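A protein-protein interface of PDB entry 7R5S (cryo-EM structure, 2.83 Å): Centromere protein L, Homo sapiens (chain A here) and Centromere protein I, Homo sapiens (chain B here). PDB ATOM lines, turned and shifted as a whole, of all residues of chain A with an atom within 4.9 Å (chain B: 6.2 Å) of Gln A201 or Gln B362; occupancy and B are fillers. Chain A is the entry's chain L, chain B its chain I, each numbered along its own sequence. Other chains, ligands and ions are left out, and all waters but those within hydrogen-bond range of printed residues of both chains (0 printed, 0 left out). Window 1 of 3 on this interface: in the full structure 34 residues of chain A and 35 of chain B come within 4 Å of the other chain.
The backbone carbonyl oxygen (O) of Pro B360 lies within hydrogen-bond range of the guanidinium group (NH2) of Arg B387 (3.3 Å).
O of Ser B361 sits at hydrogen-bond distance from NH2 of Arg B387, 3.3 Å away.
The backbone carbonyl oxygen (O) of Gln B362 sits at hydrogen-bond distance from the side-chain hydroxyl (OG) of Ser B365.
The backbone NH (N) of Gln A201 lies close to the side-chain sulfur (SG) of Cys A206 (3.8 Å).
The side-chain amide oxygen of Gln A201 sits at hydrogen-bond distance from the backbone NH of Phe A208.
Among the printed residues, pairs that only touch across the chains: Gln A201 with Gln B362 (3.8 Å), Asp A205 with Gln B362 (3.8 Å) and Asp A205 with Met B363 (3.8 Å).
OD2 of Asp A205 is in salt-bridge range of NE of Arg B387 (3.2 Å).
The side-chain carboxylate (OD2) of Asp A205 sits close to the backbone carbonyl oxygen (O) of Ser B361 (3.4 Å).
Printed residues of chain A that touch a printed residue of chain B: Gln A201 and Asp A205.
Among the printed residues, 5 pairs touch across the chains.
Gln A201 touches just one residue of chain B: Gln B362.
Gln B362 touches just these residues of chain A: Gln A201 (3.8 Å) and Asp A205 (3.8 Å).
Printed residues of chain A within 4 Å of Met B363: Asp A205 (3.8 Å).
Of the printed residues of chain A, Ser B361 touches Asp A205 (3.4 Å).
Printed residues of chain A within 4 Å of Arg B387: Asp A205.
Printed residues of chain B within 4 Å of Asp A205: Ser B361 (3.4 Å), Gln B362 (3.8 Å), Met B363 (3.8 Å) and Arg B387 (3.2 Å).
The nearest residue of chain B that does not touch Gln A201 is Ser B361 (5.6 Å).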
ATOM      1  N   GLY A 197      15.765 -27.008  20.987  1.00  0.00           N
ATOM      2  CA  GLY A 197      16.593 -26.117  21.780  1.00  0.00           C
ATOM      3  C   GLY A 197      17.240 -26.816  22.959  1.00  0.00           C
ATOM      4  O   GLY A 197      18.403 -26.558  23.279  1.00  0.00           O
ATOM      5  N   THR A 198      16.502 -27.711  23.618  1.00  0.00           N
ATOM      6  CA  THR A 198      17.074 -28.474  24.723  1.00  0.00           C
ATOM      7  C   THR A 198      18.237 -29.335  24.246  1.00  0.00           C
ATOM      8  O   THR A 198      19.297 -29.378  24.884  1.00  0.00           O
ATOM      9  CB  THR A 198      15.996 -29.339  25.375  1.00  0.00           C
ATOM     10  OG1 THR A 198      14.938 -28.503  25.860  1.00  0.00           O
ATOM     11  CG2 THR A 198      16.576 -30.134  26.534  1.00  0.00           C
ATOM     12  N   TRP A 199      18.057 -30.023  23.115  1.00  0.00           N
ATOM     13  CA  TRP A 199      19.135 -30.851  22.583  1.00  0.00           C
ATOM     14  C   TRP A 199      20.347 -30.009  22.210  1.00  0.00           C
ATOM     15  O   TRP A 199      21.487 -30.383  22.508  1.00  0.00           O
ATOM     16  CB  TRP A 199      18.644 -31.648  21.375  1.00  0.00           C
ATOM     17  CG  TRP A 199      19.638 -32.657  20.888  1.00  0.00           C
ATOM     18  CD1 TRP A 199      19.840 -33.913  21.382  1.00  0.00           C
ATOM     19  CD2 TRP A 199      20.570 -32.496  19.811  1.00  0.00           C
ATOM     20  NE1 TRP A 199      20.838 -34.543  20.681  1.00  0.00           N
ATOM     21  CE2 TRP A 199      21.302 -33.695  19.711  1.00  0.00           C
ATOM     22  CE3 TRP A 199      20.854 -31.455  18.923  1.00  0.00           C
ATOM     23  CZ2 TRP A 199      22.301 -33.882  18.758  1.00  0.00           C
ATOM     24  CZ3 TRP A 199      21.846 -31.643  17.978  1.00  0.00           C
ATOM     25  CH2 TRP A 199      22.557 -32.847  17.903  1.00  0.00           C
ATOM     26  N   PHE A 200      20.122 -28.860  21.565  1.00  0.00           N
ATOM     27  CA  PHE A 200      21.240 -28.009  21.170  1.00  0.00           C
ATOM     28  C   PHE A 200      21.981 -27.465  22.386  1.00  0.00           C
ATOM     29  O   PHE A 200      23.216 -27.412  22.396  1.00  0.00           O
ATOM     30  CB  PHE A 200      20.743 -26.864  20.287  1.00  0.00           C
ATOM     31  CG  PHE A 200      20.898 -27.123  18.816  1.00  0.00           C
ATOM     32  CD1 PHE A 200      22.065 -26.774  18.158  1.00  0.00           C
ATOM     33  CD2 PHE A 200      19.879 -27.717  18.092  1.00  0.00           C
ATOM     34  CE1 PHE A 200      22.212 -27.012  16.805  1.00  0.00           C
ATOM     35  CE2 PHE A 200      20.020 -27.957  16.739  1.00  0.00           C
ATOM     36  CZ  PHE A 200      21.187 -27.605  16.095  1.00  0.00           C
ATOM     37  N   GLN A 201      21.243 -27.064  23.424  1.00  0.00           N
ATOM     38  CA  GLN A 201      21.880 -26.547  24.630  1.00  0.00           C
ATOM     39  C   GLN A 201      22.666 -27.633  25.351  1.00  0.00           C
ATOM     40  O   GLN A 201      23.751 -27.370  25.883  1.00  0.00           O
ATOM     41  CB  GLN A 201      20.831 -25.941  25.561  1.00  0.00           C
ATOM     42  CG  GLN A 201      20.272 -24.609  25.091  1.00  0.00           C
ATOM     43  CD  GLN A 201      19.223 -24.055  26.035  1.00  0.00           C
ATOM     44  OE1 GLN A 201      18.727 -22.945  25.846  1.00  0.00           O
ATOM     45  NE2 GLN A 201      18.881 -24.828  27.058  1.00  0.00           N
ATOM     46  N   LYS A 202      22.140 -28.859  25.380  1.00  0.00           N
ATOM     47  CA  LYS A 202      22.849 -29.935  26.063  1.00  0.00           C
ATOM     48  C   LYS A 202      24.046 -30.425  25.258  1.00  0.00           C
ATOM     49  O   LYS A 202      24.999 -30.960  25.836  1.00  0.00           O
ATOM     50  CB  LYS A 202      21.896 -31.094  26.351  1.00  0.00           C
ATOM     51  CG  LYS A 202      21.025 -30.886  27.578  1.00  0.00           C
ATOM     52  CD  LYS A 202      20.176 -32.110  27.868  1.00  0.00           C
ATOM     53  CE  LYS A 202      19.490 -31.995  29.219  1.00  0.00           C
ATOM     54  NZ  LYS A 202      18.655 -30.765  29.314  1.00  0.00           N
ATOM     55  N   THR A 203      24.024 -30.251  23.937  1.00  0.00           N
ATOM     56  CA  THR A 203      25.106 -30.761  23.104  1.00  0.00           C
ATOM     57  C   THR A 203      26.233 -29.747  22.916  1.00  0.00           C
ATOM     58  O   THR A 203      27.401 -30.070  23.151  1.00  0.00           O
ATOM     59  CB  THR A 203      24.559 -31.192  21.741  1.00  0.00           C
ATOM     60  OG1 THR A 203      23.533 -32.174  21.927  1.00  0.00           O
ATOM     61  CG2 THR A 203      25.668 -31.786  20.888  1.00  0.00           C
ATOM     62  N   PHE A 204      25.906 -28.526  22.495  1.00  0.00           N
ATOM     63  CA  PHE A 204      26.916 -27.539  22.140  1.00  0.00           C
ATOM     64  C   PHE A 204      27.098 -26.449  23.187  1.00  0.00           C
ATOM     65  O   PHE A 204      27.886 -25.524  22.961  1.00  0.00           O
ATOM     66  CB  PHE A 204      26.577 -26.903  20.787  1.00  0.00           C
ATOM     67  CG  PHE A 204      26.472 -27.894  19.664  1.00  0.00           C
ATOM     68  CD1 PHE A 204      27.610 -28.403  19.064  1.00  0.00           C
ATOM     69  CD2 PHE A 204      25.235 -28.317  19.211  1.00  0.00           C
ATOM     70  CE1 PHE A 204      27.517 -29.316  18.031  1.00  0.00           C
ATOM     71  CE2 PHE A 204      25.135 -29.229  18.178  1.00  0.00           C
ATOM     72  CZ  PHE A 204      26.277 -29.729  17.589  1.00  0.00           C
ATOM     73  N   ASP A 205      26.395 -26.530  24.318  1.00  0.00           N
ATOM     74  CA  ASP A 205      26.536 -25.577  25.421  1.00  0.00           C
ATOM     75  C   ASP A 205      26.260 -24.146  24.951  1.00  0.00           C
ATOM     76  O   ASP A 205      27.123 -23.268  24.989  1.00  0.00           O
ATOM     77  CB  ASP A 205      27.923 -25.693  26.066  1.00  0.00           C
ATOM     78  CG  ASP A 205      28.009 -24.981  27.403  1.00  0.00           C
ATOM     79  OD1 ASP A 205      26.969 -24.489  27.888  1.00  0.00           O
ATOM     80  OD2 ASP A 205      29.120 -24.914  27.969  1.00  0.00           O
ATOM     81  N   CYS A 206      25.029 -23.929  24.503  1.00  0.00           N
ATOM     82  CA  CYS A 206      24.573 -22.631  24.024  1.00  0.00           C
ATOM     83  C   CYS A 206      23.386 -22.164  24.863  1.00  0.00           C
ATOM     84  O   CYS A 206      22.984 -22.815  25.829  1.00  0.00           O
ATOM     85  CB  CYS A 206      24.207 -22.699  22.539  1.00  0.00           C
ATOM     86  SG  CYS A 206      23.197 -24.122  22.080  1.00  0.00           S
ATOM     87  N   TYR A 207      22.826 -21.017  24.482  1.00  0.00           N
ATOM     88  CA  TYR A 207      21.727 -20.405  25.222  1.00  0.00           C
ATOM     89  C   TYR A 207      20.795 -19.712  24.240  1.00  0.00           C
ATOM     90  O   TYR A 207      21.221 -18.817  23.507  1.00  0.00           O
ATOM     91  CB  TYR A 207      22.254 -19.408  26.259  1.00  0.00           C
ATOM     92  CG  TYR A 207      21.301 -19.141  27.403  1.00  0.00           C
ATOM     93  CD1 TYR A 207      20.277 -18.212  27.278  1.00  0.00           C
ATOM     94  CD2 TYR A 207      21.432 -19.813  28.610  1.00  0.00           C
ATOM     95  CE1 TYR A 207      19.406 -17.964  28.320  1.00  0.00           C
ATOM     96  CE2 TYR A 207      20.566 -19.572  29.660  1.00  0.00           C
ATOM     97  CZ  TYR A 207      19.556 -18.646  29.509  1.00  0.00           C
ATOM     98  OH  TYR A 207      18.691 -18.402  30.551  1.00  0.00           O
ATOM     99  N   PHE A 208      19.531 -20.125  24.230  1.00  0.00           N
ATOM    100  CA  PHE A 208      18.508 -19.516  23.393  1.00  0.00           C
ATOM    101  C   PHE A 208      17.732 -18.485  24.199  1.00  0.00           C
ATOM    102  O   PHE A 208      17.352 -18.739  25.346  1.00  0.00           O
ATOM    103  CB  PHE A 208      17.545 -20.571  22.843  1.00  0.00           C
ATOM    104  CG  PHE A 208      18.169 -21.509  21.850  1.00  0.00           C
ATOM    105  CD1 PHE A 208      18.865 -22.628  22.274  1.00  0.00           C
ATOM    106  CD2 PHE A 208      18.048 -21.279  20.490  1.00  0.00           C
ATOM    107  CE1 PHE A 208      19.436 -23.494  21.363  1.00  0.00           C
ATOM    108  CE2 PHE A 208      18.616 -22.141  19.573  1.00  0.00           C
ATOM    109  CZ  PHE A 208      19.310 -23.250  20.010  1.00  0.00           C
ATOM    110  N   PRO B 311      22.778 -25.921  35.674  1.00  0.00           N
ATOM    111  CA  PRO B 311      22.672 -27.183  34.935  1.00  0.00           C
ATOM    112  C   PRO B 311      23.099 -28.373  35.782  1.00  0.00           C
ATOM    113  O   PRO B 311      23.792 -28.241  36.794  1.00  0.00           O
ATOM    114  CB  PRO B 311      23.619 -26.981  33.745  1.00  0.00           C
ATOM    115  CG  PRO B 311      23.758 -25.500  33.613  1.00  0.00           C
ATOM    116  CD  PRO B 311      23.673 -24.962  35.007  1.00  0.00           C
ATOM    117  N   VAL B 312      22.670 -29.554  35.349  1.00  0.00           N
ATOM    118  CA  VAL B 312      22.972 -30.788  36.056  1.00  0.00           C
ATOM    119  C   VAL B 312      24.343 -31.295  35.625  1.00  0.00           C
ATOM    120  O   VAL B 312      24.847 -30.972  34.547  1.00  0.00           O
ATOM    121  CB  VAL B 312      21.887 -31.856  35.818  1.00  0.00           C
ATOM    122  CG1 VAL B 312      20.578 -31.434  36.466  1.00  0.00           C
ATOM    123  CG2 VAL B 312      21.697 -32.095  34.329  1.00  0.00           C
ATOM    124  N   ASN B 314      26.769 -33.651  34.067  1.00  0.00           N
ATOM    125  CA  ASN B 314      26.756 -34.688  33.046  1.00  0.00           C
ATOM    126  C   ASN B 314      28.129 -34.772  32.398  1.00  0.00           C
ATOM    127  O   ASN B 314      28.923 -33.830  32.452  1.00  0.00           O
ATOM    128  CB  ASN B 314      25.685 -34.423  31.979  1.00  0.00           C
ATOM    129  CG  ASN B 314      24.286 -34.748  32.462  1.00  0.00           C
ATOM    130  OD1 ASN B 314      24.087 -35.673  33.249  1.00  0.00           O
ATOM    131  ND2 ASN B 314      23.306 -33.986  31.991  1.00  0.00           N
ATOM    132  N   SER B 315      28.401 -35.917  31.779  1.00  0.00           N
ATOM    133  CA  SER B 315      29.665 -36.112  31.089  1.00  0.00           C
ATOM    134  C   SER B 315      29.727 -35.241  29.837  1.00  0.00           C
ATOM    135  O   SER B 315      28.763 -34.568  29.460  1.00  0.00           O
ATOM    136  CB  SER B 315      29.854 -37.584  30.725  1.00  0.00           C
ATOM    137  OG  SER B 315      30.129 -38.365  31.875  1.00  0.00           O
ATOM    138  N   PRO B 360      32.965 -30.925  32.094  1.00  0.00           N
ATOM    139  CA  PRO B 360      31.539 -31.181  31.863  1.00  0.00           C
ATOM    140  C   PRO B 360      31.081 -30.636  30.519  1.00  0.00           C
ATOM    141  O   PRO B 360      31.778 -29.878  29.842  1.00  0.00           O
ATOM    142  CB  PRO B 360      30.852 -30.450  33.020  1.00  0.00           C
ATOM    143  CG  PRO B 360      31.921 -30.254  34.049  1.00  0.00           C
ATOM    144  CD  PRO B 360      33.188 -30.080  33.276  1.00  0.00           C
ATOM    145  N   SER B 361      29.870 -31.044  30.134  1.00  0.00           N
ATOM    146  CA  SER B 361      29.278 -30.531  28.903  1.00  0.00           C
ATOM    147  C   SER B 361      28.783 -29.103  29.078  1.00  0.00           C
ATOM    148  O   SER B 361      28.808 -28.317  28.123  1.00  0.00           O
ATOM    149  CB  SER B 361      28.136 -31.440  28.450  1.00  0.00           C
ATOM    150  OG  SER B 361      27.093 -31.465  29.407  1.00  0.00           O
ATOM    151  N   GLN B 362      28.330 -28.750  30.278  1.00  0.00           N
ATOM    152  CA  GLN B 362      27.902 -27.396  30.604  1.00  0.00           C
ATOM    153  C   GLN B 362      28.713 -26.912  31.796  1.00  0.00           C
ATOM    154  O   GLN B 362      28.707 -27.551  32.854  1.00  0.00           O
ATOM    155  CB  GLN B 362      26.403 -27.350  30.904  1.00  0.00           C
ATOM    156  CG  GLN B 362      25.528 -27.693  29.710  1.00  0.00           C
ATOM    157  CD  GLN B 362      24.049 -27.679  30.042  1.00  0.00           C
ATOM    158  OE1 GLN B 362      23.323 -26.766  29.654  1.00  0.00           O
ATOM    159  NE2 GLN B 362      23.597 -28.697  30.763  1.00  0.00           N
ATOM    160  N   MET B 363      29.409 -25.787  31.624  1.00  0.00           N
ATOM    161  CA  MET B 363      30.321 -25.302  32.653  1.00  0.00           C
ATOM    162  C   MET B 363      29.595 -24.813  33.900  1.00  0.00           C
ATOM    163  O   MET B 363      30.204 -24.763  34.974  1.00  0.00           O
ATOM    164  CB  MET B 363      31.201 -24.187  32.087  1.00  0.00           C
ATOM    165  CG  MET B 363      32.520 -24.005  32.817  1.00  0.00           C
ATOM    166  SD  MET B 363      33.529 -25.500  32.816  1.00  0.00           S
ATOM    167  CE  MET B 363      33.679 -25.810  31.059  1.00  0.00           C
ATOM    168  N   GLY B 364      28.313 -24.456  33.786  1.00  0.00           N
ATOM    169  CA  GLY B 364      27.579 -23.979  34.947  1.00  0.00           C
ATOM    170  C   GLY B 364      27.531 -24.982  36.082  1.00  0.00           C
ATOM    171  O   GLY B 364      27.491 -24.597  37.255  1.00  0.00           O
ATOM    172  N   SER B 365      27.547 -26.278  35.757  1.00  0.00           N
ATOM    173  CA  SER B 365      27.535 -27.311  36.787  1.00  0.00           C
ATOM    174  C   SER B 365      28.777 -27.264  37.667  1.00  0.00           C
ATOM    175  O   SER B 365      28.771 -27.843  38.759  1.00  0.00           O
ATOM    176  CB  SER B 365      27.405 -28.690  36.142  1.00  0.00           C
ATOM    177  OG  SER B 365      28.268 -28.814  35.025  1.00  0.00           O
ATOM    178  N   VAL B 366      29.841 -26.593  37.219  1.00  0.00           N
ATOM    179  CA  VAL B 366      31.029 -26.434  38.049  1.00  0.00           C
ATOM    180  C   VAL B 366      30.762 -25.502  39.227  1.00  0.00           C
ATOM    181  O   VAL B 366      31.488 -25.546  40.227  1.00  0.00           O
ATOM    182  CB  VAL B 366      32.198 -25.932  37.177  1.00  0.00           C
ATOM    183  CG1 VAL B 366      33.480 -25.801  37.985  1.00  0.00           C
ATOM    184  CG2 VAL B 366      32.415 -26.871  36.002  1.00  0.00           C
ATOM    185  N   ARG B 387      32.980 -19.729  27.882  1.00  0.00           N
ATOM    186  CA  ARG B 387      31.732 -20.455  28.099  1.00  0.00           C
ATOM    187  C   ARG B 387      31.083 -20.045  29.414  1.00  0.00           C
ATOM    188  O   ARG B 387      29.875 -19.769  29.470  1.00  0.00           O
ATOM    189  CB  ARG B 387      31.992 -21.962  28.072  1.00  0.00           C
ATOM    190  CG  ARG B 387      32.421 -22.495  26.716  1.00  0.00           C
ATOM    191  CD  ARG B 387      33.125 -23.836  26.843  1.00  0.00           C
ATOM    192  NE  ARG B 387      32.264 -24.856  27.433  1.00  0.00           N
ATOM    193  CZ  ARG B 387      32.648 -26.104  27.681  1.00  0.00           C
ATOM    194  NH1 ARG B 387      33.882 -26.489  27.392  1.00  0.00           N
ATOM    195  NH2 ARG B 387      31.797 -26.966  28.220  1.00  0.00           N
ATOM    196  N   TRP B 391      27.421 -18.118  29.811  1.00  0.00           N
ATOM    197  CA  TRP B 391      26.349 -18.734  30.587  1.00  0.00           C
ATOM    198  C   TRP B 391      25.934 -17.850  31.757  1.00  0.00           C
ATOM    199  O   TRP B 391      24.742 -17.593  31.965  1.00  0.00           O
ATOM    200  CB  TRP B 391      26.777 -20.113  31.085  1.00  0.00           C
ATOM    201  CG  TRP B 391      25.816 -20.693  32.075  1.00  0.00           C
ATOM    202  CD1 TRP B 391      24.644 -21.336  31.800  1.00  0.00           C
ATOM    203  CD2 TRP B 391      25.934 -20.671  33.503  1.00  0.00           C
ATOM    204  NE1 TRP B 391      24.029 -21.718  32.967  1.00  0.00           N
ATOM    205  CE2 TRP B 391      24.800 -21.323  34.026  1.00  0.00           C
ATOM    206  CE3 TRP B 391      26.891 -20.167  34.389  1.00  0.00           C
ATOM    207  CZ2 TRP B 391      24.597 -21.483  35.395  1.00  0.00           C
ATOM    208  CZ3 TRP B 391      26.687 -20.326  35.746  1.00  0.00           C
ATOM    209  CH2 TRP B 391      25.549 -20.979  36.236  1.00  0.00           C
